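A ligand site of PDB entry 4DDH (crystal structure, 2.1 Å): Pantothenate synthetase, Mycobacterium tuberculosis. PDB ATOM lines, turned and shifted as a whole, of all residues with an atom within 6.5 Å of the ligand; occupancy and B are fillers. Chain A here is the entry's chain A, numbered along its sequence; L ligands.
A ring nitrogen (ND1) of His 47 lies within hydrogen-bond range of the backbone NH (N) of His 44 (3.0 Å).
OG of Ser 196 lies within hydrogen-bond range of N of Arg 198, at 2.8 Å.
A ring nitrogen (ND1) of His 44 sits at hydrogen-bond distance from the backbone NH (N) of Gly 46, 2.8 Å away.
O of Val 187 sits close to N of Met 195 (3.1 Å).
The side-chain hydroxyl (OG) of Ser 197 sits close to the guanidinium group (NE) of Arg 198, at 2.6 Å.
The side-chain hydroxyl of Ser 197 lies within hydrogen-bond range of the side-chain hydroxyl of Tyr 82, at 3.1 Å.
The backbone NH of Lys 160 is in hydrogen-bond range of the side-chain hydroxyl of Thr 186 (3.1 Å).
NZ of Lys 160 lies within salt-bridge range of OD1 of Asp 161 (2.9 Å).
Gly 46 touches the ligand (O to C11, 3.4 Å).
His 47 touches the ligand.
OD2 of Asp 161 touches C5 of the ligand, 3.5 Å away.
Pro 185 touches the ligand.
Thr 186 touches the ligand.
Met 195 touches the ligand (O to C7, 3.2 Å).
Hydrophobic or aromatic side chains within 4 Å of the ligand: His 44, His 47 and Val 187.
Of the 27 residues printed, 11 come within 4 Å of the ligand.
The nearest printed residue that does not touch the ligand is Gly 158 (4.1 Å).
O4 of the ligand sits at hydrogen-bond distance from N of Val 187.
The side-chain amino group of Lys 160 lies within salt-bridge range of an oxygen (O2) of the ligand, 2.8 Å away.
O2 of the ligand lies within hydrogen-bond range of OG of Ser 196.
An oxygen (O3) of the ligand lies within hydrogen-bond range of a ring nitrogen (NE2) of His 44 (2.6 Å).
N of Ser 197 sits at hydrogen-bond distance from O3 of the ligand (2.8 Å).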
ATOM      1  N   PRO A  38      -2.025  25.580   4.910  1.00  0.00           N
ATOM      2  CA  PRO A  38      -1.949  25.589   6.383  1.00  0.00           C
ATOM      3  C   PRO A  38      -2.003  24.181   6.861  1.00  0.00           C
ATOM      4  O   PRO A  38      -2.927  23.436   6.494  1.00  0.00           O
ATOM      5  CB  PRO A  38      -3.283  26.240   6.821  1.00  0.00           C
ATOM      6  CG  PRO A  38      -3.852  26.861   5.576  1.00  0.00           C
ATOM      7  CD  PRO A  38      -3.359  25.944   4.442  1.00  0.00           C
ATOM      8  N   THR A  39      -1.078  23.798   7.724  1.00  0.00           N
ATOM      9  CA  THR A  39      -1.129  22.422   8.242  1.00  0.00           C
ATOM     10  C   THR A  39      -0.794  22.362   9.744  1.00  0.00           C
ATOM     11  O   THR A  39      -0.328  23.357  10.349  1.00  0.00           O
ATOM     12  CB  THR A  39      -0.045  21.455   7.484  1.00  0.00           C
ATOM     13  OG1 THR A  39       1.243  21.695   8.038  1.00  0.00           O
ATOM     14  CG2 THR A  39       0.102  21.770   5.998  1.00  0.00           C
ATOM     15  N   GLY A  41       1.425  19.974  10.643  1.00  0.00           N
ATOM     16  CA  GLY A  41       2.613  19.049  10.506  1.00  0.00           C
ATOM     17  C   GLY A  41       2.166  17.561  10.450  1.00  0.00           C
ATOM     18  O   GLY A  41       0.965  17.254  10.134  1.00  0.00           O
ATOM     19  N   ALA A  42       3.117  16.665  10.750  1.00  0.00           N
ATOM     20  CA  ALA A  42       2.967  15.234  10.504  1.00  0.00           C
ATOM     21  C   ALA A  42       2.536  15.009   9.060  1.00  0.00           C
ATOM     22  O   ALA A  42       1.499  14.452   8.781  1.00  0.00           O
ATOM     23  CB  ALA A  42       1.952  14.647  11.491  1.00  0.00           C
ATOM     24  N   HIS A  44       1.859  13.960   5.340  1.00  0.00           N
ATOM     25  CA  HIS A  44       1.737  12.723   4.611  1.00  0.00           C
ATOM     26  C   HIS A  44       1.427  13.095   3.157  1.00  0.00           C
ATOM     27  O   HIS A  44       1.502  14.277   2.742  1.00  0.00           O
ATOM     28  CB  HIS A  44       0.605  11.914   5.223  1.00  0.00           C
ATOM     29  CG  HIS A  44      -0.682  12.698   5.386  1.00  0.00           C
ATOM     30  ND1 HIS A  44      -1.454  13.076   4.304  1.00  0.00           N
ATOM     31  CD2 HIS A  44      -1.341  13.113   6.486  1.00  0.00           C
ATOM     32  CE1 HIS A  44      -2.512  13.753   4.732  1.00  0.00           C
ATOM     33  NE2 HIS A  44      -2.472  13.788   6.056  1.00  0.00           N
ATOM     34  N   GLU A  45       1.159  12.087   2.366  1.00  0.00           N
ATOM     35  CA  GLU A  45       0.870  12.268   0.963  1.00  0.00           C
ATOM     36  C   GLU A  45      -0.312  13.219   0.633  1.00  0.00           C
ATOM     37  O   GLU A  45      -0.308  13.920  -0.417  1.00  0.00           O
ATOM     38  CB  GLU A  45       0.619  10.870   0.367  1.00  0.00           C
ATOM     39  CG  GLU A  45       0.701  10.865  -1.118  1.00  0.00           C
ATOM     40  CD  GLU A  45       2.090  11.266  -1.658  1.00  0.00           C
ATOM     41  OE1 GLU A  45       3.152  11.122  -0.942  1.00  0.00           O
ATOM     42  OE2 GLU A  45       2.110  11.704  -2.834  1.00  0.00           O
ATOM     43  N   GLY A  46      -1.350  13.238   1.464  1.00  0.00           N
ATOM     44  CA  GLY A  46      -2.445  14.219   1.226  1.00  0.00           C
ATOM     45  C   GLY A  46      -1.963  15.666   1.340  1.00  0.00           C
ATOM     46  O   GLY A  46      -2.383  16.496   0.589  1.00  0.00           O
ATOM     47  N   HIS A  47      -1.113  15.971   2.349  1.00  0.00           N
ATOM     48  CA  HIS A  47      -0.523  17.278   2.411  1.00  0.00           C
ATOM     49  C   HIS A  47       0.291  17.528   1.169  1.00  0.00           C
ATOM     50  O   HIS A  47       0.365  18.650   0.732  1.00  0.00           O
ATOM     51  CB  HIS A  47       0.441  17.468   3.602  1.00  0.00           C
ATOM     52  CG  HIS A  47      -0.223  17.317   4.907  1.00  0.00           C
ATOM     53  ND1 HIS A  47      -0.047  16.229   5.703  1.00  0.00           N
ATOM     54  CD2 HIS A  47      -1.123  18.117   5.539  1.00  0.00           C
ATOM     55  CE1 HIS A  47      -0.794  16.350   6.790  1.00  0.00           C
ATOM     56  NE2 HIS A  47      -1.478  17.484   6.700  1.00  0.00           N
ATOM     57  N   LEU A  48       0.930  16.499   0.613  1.00  0.00           N
ATOM     58  CA  LEU A  48       1.749  16.787  -0.597  1.00  0.00           C
ATOM     59  C   LEU A  48       0.877  17.070  -1.802  1.00  0.00           C
ATOM     60  O   LEU A  48       1.282  17.785  -2.724  1.00  0.00           O
ATOM     61  CB  LEU A  48       2.716  15.643  -0.862  1.00  0.00           C
ATOM     62  CG  LEU A  48       3.708  15.582   0.295  1.00  0.00           C
ATOM     63  CD1 LEU A  48       4.380  14.207   0.438  1.00  0.00           C
ATOM     64  CD2 LEU A  48       4.747  16.623   0.091  1.00  0.00           C
ATOM     65  N   ALA A  49      -0.347  16.584  -1.793  1.00  0.00           N
ATOM     66  CA  ALA A  49      -1.228  16.912  -2.925  1.00  0.00           C
ATOM     67  C   ALA A  49      -1.600  18.370  -2.838  1.00  0.00           C
ATOM     68  O   ALA A  49      -1.723  19.066  -3.879  1.00  0.00           O
ATOM     69  CB  ALA A  49      -2.484  16.058  -2.943  1.00  0.00           C
ATOM     70  N   LEU A  50      -1.790  18.870  -1.611  1.00  0.00           N
ATOM     71  CA  LEU A  50      -2.048  20.293  -1.437  1.00  0.00           C
ATOM     72  C   LEU A  50      -0.906  21.126  -2.000  1.00  0.00           C
ATOM     73  O   LEU A  50      -1.150  22.052  -2.736  1.00  0.00           O
ATOM     74  CB  LEU A  50      -2.271  20.661   0.044  1.00  0.00           C
ATOM     75  CG  LEU A  50      -3.375  19.941   0.842  1.00  0.00           C
ATOM     76  CD1 LEU A  50      -3.653  20.680   2.141  1.00  0.00           C
ATOM     77  CD2 LEU A  50      -4.681  19.794   0.039  1.00  0.00           C
ATOM     78  N   TYR A  82      -0.966  14.590  19.963  1.00  0.00           N
ATOM     79  CA  TYR A  82      -0.821  14.880  18.523  1.00  0.00           C
ATOM     80  C   TYR A  82       0.572  14.540  17.958  1.00  0.00           C
ATOM     81  O   TYR A  82       1.576  14.955  18.549  1.00  0.00           O
ATOM     82  CB  TYR A  82      -1.186  16.335  18.160  1.00  0.00           C
ATOM     83  CG  TYR A  82      -1.643  16.420  16.678  1.00  0.00           C
ATOM     84  CD1 TYR A  82      -2.969  16.133  16.325  1.00  0.00           C
ATOM     85  CD2 TYR A  82      -0.759  16.737  15.658  1.00  0.00           C
ATOM     86  CE1 TYR A  82      -3.380  16.180  14.974  1.00  0.00           C
ATOM     87  CE2 TYR A  82      -1.177  16.757  14.309  1.00  0.00           C
ATOM     88  CZ  TYR A  82      -2.490  16.465  14.008  1.00  0.00           C
ATOM     89  OH  TYR A  82      -2.955  16.494  12.718  1.00  0.00           O
ATOM     90  N   PHE A 157      -6.996  23.467   1.135  1.00  0.00           N
ATOM     91  CA  PHE A 157      -7.390  22.478   2.117  1.00  0.00           C
ATOM     92  C   PHE A 157      -7.804  21.179   1.443  1.00  0.00           C
ATOM     93  O   PHE A 157      -8.303  21.185   0.294  1.00  0.00           O
ATOM     94  CB  PHE A 157      -8.561  23.015   2.992  1.00  0.00           C
ATOM     95  CG  PHE A 157      -8.191  24.187   3.854  1.00  0.00           C
ATOM     96  CD1 PHE A 157      -7.664  23.989   5.148  1.00  0.00           C
ATOM     97  CD2 PHE A 157      -8.429  25.489   3.435  1.00  0.00           C
ATOM     98  CE1 PHE A 157      -7.318  25.118   5.955  1.00  0.00           C
ATOM     99  CE2 PHE A 157      -8.145  26.575   4.241  1.00  0.00           C
ATOM    100  CZ  PHE A 157      -7.542  26.397   5.469  1.00  0.00           C
ATOM    101  N   GLY A 158      -7.595  20.082   2.136  1.00  0.00           N
ATOM    102  CA  GLY A 158      -8.165  18.800   1.729  1.00  0.00           C
ATOM    103  C   GLY A 158      -9.669  18.649   1.943  1.00  0.00           C
ATOM    104  O   GLY A 158     -10.227  19.195   2.904  1.00  0.00           O
ATOM    105  N   GLU A 159     -10.315  17.846   1.090  1.00  0.00           N
ATOM    106  CA  GLU A 159     -11.745  17.478   1.299  1.00  0.00           C
ATOM    107  C   GLU A 159     -11.952  16.439   2.421  1.00  0.00           C
ATOM    108  O   GLU A 159     -13.102  16.222   2.895  1.00  0.00           O
ATOM    109  CB  GLU A 159     -12.382  16.986  -0.002  1.00  0.00           C
ATOM    110  CG  GLU A 159     -12.274  17.989  -1.145  1.00  0.00           C
ATOM    111  CD  GLU A 159     -13.005  17.464  -2.425  1.00  0.00           C
ATOM    112  OE1 GLU A 159     -13.323  16.251  -2.497  1.00  0.00           O
ATOM    113  OE2 GLU A 159     -13.179  18.270  -3.354  1.00  0.00           O
ATOM    114  N   LYS A 160     -10.875  15.825   2.897  1.00  0.00           N
ATOM    115  CA  LYS A 160     -11.029  14.831   3.927  1.00  0.00           C
ATOM    116  C   LYS A 160     -11.797  15.422   5.146  1.00  0.00           C
ATOM    117  O   LYS A 160     -12.736  14.797   5.651  1.00  0.00           O
ATOM    118  CB  LYS A 160      -9.678  14.204   4.347  1.00  0.00           C
ATOM    119  CG  LYS A 160      -9.801  12.896   5.214  1.00  0.00           C
ATOM    120  CD  LYS A 160      -9.928  13.111   6.708  1.00  0.00           C
ATOM    121  CE  LYS A 160      -8.628  13.396   7.409  1.00  0.00           C
ATOM    122  NZ  LYS A 160      -8.791  14.013   8.805  1.00  0.00           N
ATOM    123  N   ASP A 161     -11.398  16.609   5.581  1.00  0.00           N
ATOM    124  CA  ASP A 161     -12.065  17.296   6.672  1.00  0.00           C
ATOM    125  C   ASP A 161     -13.067  18.238   6.061  1.00  0.00           C
ATOM    126  O   ASP A 161     -12.916  19.441   6.045  1.00  0.00           O
ATOM    127  CB  ASP A 161     -11.069  18.033   7.505  1.00  0.00           C
ATOM    128  CG  ASP A 161     -10.106  17.073   8.221  1.00  0.00           C
ATOM    129  OD1 ASP A 161     -10.572  16.307   9.043  1.00  0.00           O
ATOM    130  OD2 ASP A 161      -8.899  17.110   7.938  1.00  0.00           O
ATOM    131  N   VAL A 184      -9.085  20.239  -2.053  1.00  0.00           N
ATOM    132  CA  VAL A 184      -8.337  19.324  -2.839  1.00  0.00           C
ATOM    133  C   VAL A 184      -8.838  17.938  -2.540  1.00  0.00           C
ATOM    134  O   VAL A 184      -9.039  17.531  -1.358  1.00  0.00           O
ATOM    135  CB  VAL A 184      -6.795  19.497  -2.600  1.00  0.00           C
ATOM    136  CG1 VAL A 184      -5.941  18.444  -3.409  1.00  0.00           C
ATOM    137  CG2 VAL A 184      -6.440  20.823  -2.994  1.00  0.00           C
ATOM    138  N   PRO A 185      -9.095  17.167  -3.613  1.00  0.00           N
ATOM    139  CA  PRO A 185      -9.648  15.815  -3.330  1.00  0.00           C
ATOM    140  C   PRO A 185      -8.737  14.947  -2.451  1.00  0.00           C
ATOM    141  O   PRO A 185      -7.503  15.003  -2.591  1.00  0.00           O
ATOM    142  CB  PRO A 185      -9.853  15.216  -4.724  1.00  0.00           C
ATOM    143  CG  PRO A 185     -10.053  16.463  -5.691  1.00  0.00           C
ATOM    144  CD  PRO A 185      -9.100  17.515  -5.068  1.00  0.00           C
ATOM    145  N   THR A 186      -9.345  14.193  -1.547  1.00  0.00           N
ATOM    146  CA  THR A 186      -8.688  13.255  -0.594  1.00  0.00           C
ATOM    147  C   THR A 186      -7.773  12.219  -1.291  1.00  0.00           C
ATOM    148  O   THR A 186      -8.220  11.496  -2.175  1.00  0.00           O
ATOM    149  CB  THR A 186      -9.819  12.558   0.135  1.00  0.00           C
ATOM    150  OG1 THR A 186     -10.566  13.560   0.832  1.00  0.00           O
ATOM    151  CG2 THR A 186      -9.399  11.470   1.128  1.00  0.00           C
ATOM    152  N   VAL A 187      -6.504  12.185  -0.923  1.00  0.00           N
ATOM    153  CA  VAL A 187      -5.575  11.138  -1.346  1.00  0.00           C
ATOM    154  C   VAL A 187      -5.903   9.889  -0.471  1.00  0.00           C
ATOM    155  O   VAL A 187      -6.170   9.996   0.719  1.00  0.00           O
ATOM    156  CB  VAL A 187      -4.042  11.558  -1.150  1.00  0.00           C
ATOM    157  CG1 VAL A 187      -3.102  10.430  -1.648  1.00  0.00           C
ATOM    158  CG2 VAL A 187      -3.679  12.862  -1.876  1.00  0.00           C
ATOM    159  N   ARG A 188      -5.931   8.719  -1.090  1.00  0.00           N
ATOM    160  CA  ARG A 188      -6.296   7.488  -0.371  1.00  0.00           C
ATOM    161  C   ARG A 188      -5.172   6.460  -0.518  1.00  0.00           C
ATOM    162  O   ARG A 188      -4.392   6.589  -1.486  1.00  0.00           O
ATOM    163  CB  ARG A 188      -7.573   6.920  -0.975  1.00  0.00           C
ATOM    164  CG  ARG A 188      -8.670   7.998  -0.938  1.00  0.00           C
ATOM    165  CD  ARG A 188      -9.992   7.490  -1.560  1.00  0.00           C
ATOM    166  NE  ARG A 188     -11.013   8.468  -1.182  1.00  0.00           N
ATOM    167  CZ  ARG A 188     -11.740   8.435  -0.054  1.00  0.00           C
ATOM    168  NH1 ARG A 188     -11.584   7.439   0.823  1.00  0.00           N
ATOM    169  NH2 ARG A 188     -12.618   9.426   0.208  1.00  0.00           N
ATOM    170  N   ALA A 194      -8.758   6.730   3.491  1.00  0.00           N
ATOM    171  CA  ALA A 194      -8.373   8.175   3.466  1.00  0.00           C
ATOM    172  C   ALA A 194      -7.075   8.427   4.285  1.00  0.00           C
ATOM    173  O   ALA A 194      -6.928   7.929   5.414  1.00  0.00           O
ATOM    174  CB  ALA A 194      -9.481   9.083   3.985  1.00  0.00           C
ATOM    175  N   MET A 195      -6.172   9.199   3.689  1.00  0.00           N
ATOM    176  CA  MET A 195      -4.932   9.607   4.363  1.00  0.00           C
ATOM    177  C   MET A 195      -5.262  10.531   5.528  1.00  0.00           C
ATOM    178  O   MET A 195      -6.163  11.394   5.416  1.00  0.00           O
ATOM    179  CB  MET A 195      -4.045  10.375   3.415  1.00  0.00           C
ATOM    180  CG  MET A 195      -3.761   9.594   2.150  1.00  0.00           C
ATOM    181  SD  MET A 195      -2.075   9.053   2.061  1.00  0.00           S
ATOM    182  CE  MET A 195      -1.988   8.234   3.626  1.00  0.00           C
ATOM    183  N   SER A 196      -4.544  10.328   6.629  1.00  0.00           N
ATOM    184  CA  SER A 196      -4.728  11.128   7.795  1.00  0.00           C
ATOM    185  C   SER A 196      -3.483  10.923   8.665  1.00  0.00           C
ATOM    186  O   SER A 196      -2.915   9.836   8.702  1.00  0.00           O
ATOM    187  CB  SER A 196      -6.030  10.669   8.515  1.00  0.00           C
ATOM    188  OG  SER A 196      -5.939  10.830   9.916  1.00  0.00           O
ATOM    189  N   SER A 197      -3.081  11.998   9.342  1.00  0.00           N
ATOM    190  CA  SER A 197      -1.987  11.973  10.269  1.00  0.00           C
ATOM    191  C   SER A 197      -2.299  10.915  11.289  1.00  0.00           C
ATOM    192  O   SER A 197      -1.384  10.319  11.846  1.00  0.00           O
ATOM    193  CB  SER A 197      -1.894  13.304  10.999  1.00  0.00           C
ATOM    194  OG  SER A 197      -3.005  13.468  11.857  1.00  0.00           O
ATOM    195  N   ARG A 198      -3.593  10.646  11.503  1.00  0.00           N
ATOM    196  CA  ARG A 198      -3.952   9.781  12.596  1.00  0.00           C
ATOM    197  C   ARG A 198      -4.118   8.292  12.220  1.00  0.00           C
ATOM    198  O   ARG A 198      -4.353   7.418  13.135  1.00  0.00           O
ATOM    199  CB  ARG A 198      -5.163  10.348  13.363  1.00  0.00           C
ATOM    200  CG  ARG A 198      -4.828  11.461  14.379  1.00  0.00           C
ATOM    201  CD  ARG A 198      -4.268  12.731  13.741  1.00  0.00           C
ATOM    202  NE  ARG A 198      -5.266  13.598  13.125  1.00  0.00           N
ATOM    203  CZ  ARG A 198      -6.350  14.057  13.753  1.00  0.00           C
ATOM    204  NH1 ARG A 198      -7.196  14.856  13.117  1.00  0.00           N
ATOM    205  NH2 ARG A 198      -6.593  13.688  15.005  1.00  0.00           N
HETATM  206  O1  LIG L   1      -4.609  17.673   4.786  1.00  0.00           O
HETATM  207  C1  LIG L   1      -5.098  16.539   4.114  1.00  0.00           C
HETATM  208  C2  LIG L   1      -5.511  15.693   5.100  1.00  0.00           C
HETATM  209  C3  LIG L   1      -5.275  16.312   6.295  1.00  0.00           C
HETATM  210  C4  LIG L   1      -4.756  17.527   6.103  1.00  0.00           C
HETATM  211  C5  LIG L   1      -5.665  15.871   7.747  1.00  0.00           C
HETATM  212  C6  LIG L   1      -5.120  14.637   8.319  1.00  0.00           C
HETATM  213  O2  LIG L   1      -5.958  14.017   9.006  1.00  0.00           O
HETATM  214  O3  LIG L   1      -3.896  14.381   8.163  1.00  0.00           O
HETATM  215  C7  LIG L   1      -6.011  14.480   4.758  1.00  0.00           C
HETATM  216  C8  LIG L   1      -6.122  14.089   3.416  1.00  0.00           C
HETATM  217  C9  LIG L   1      -5.709  14.971   2.419  1.00  0.00           C
HETATM  218  C10 LIG L   1      -5.163  16.226   2.797  1.00  0.00           C
HETATM  219  O4  LIG L   1      -5.854  14.591   1.114  1.00  0.00           O
HETATM  220  C11 LIG L   1      -5.632  15.655   0.163  1.00  0.00           C
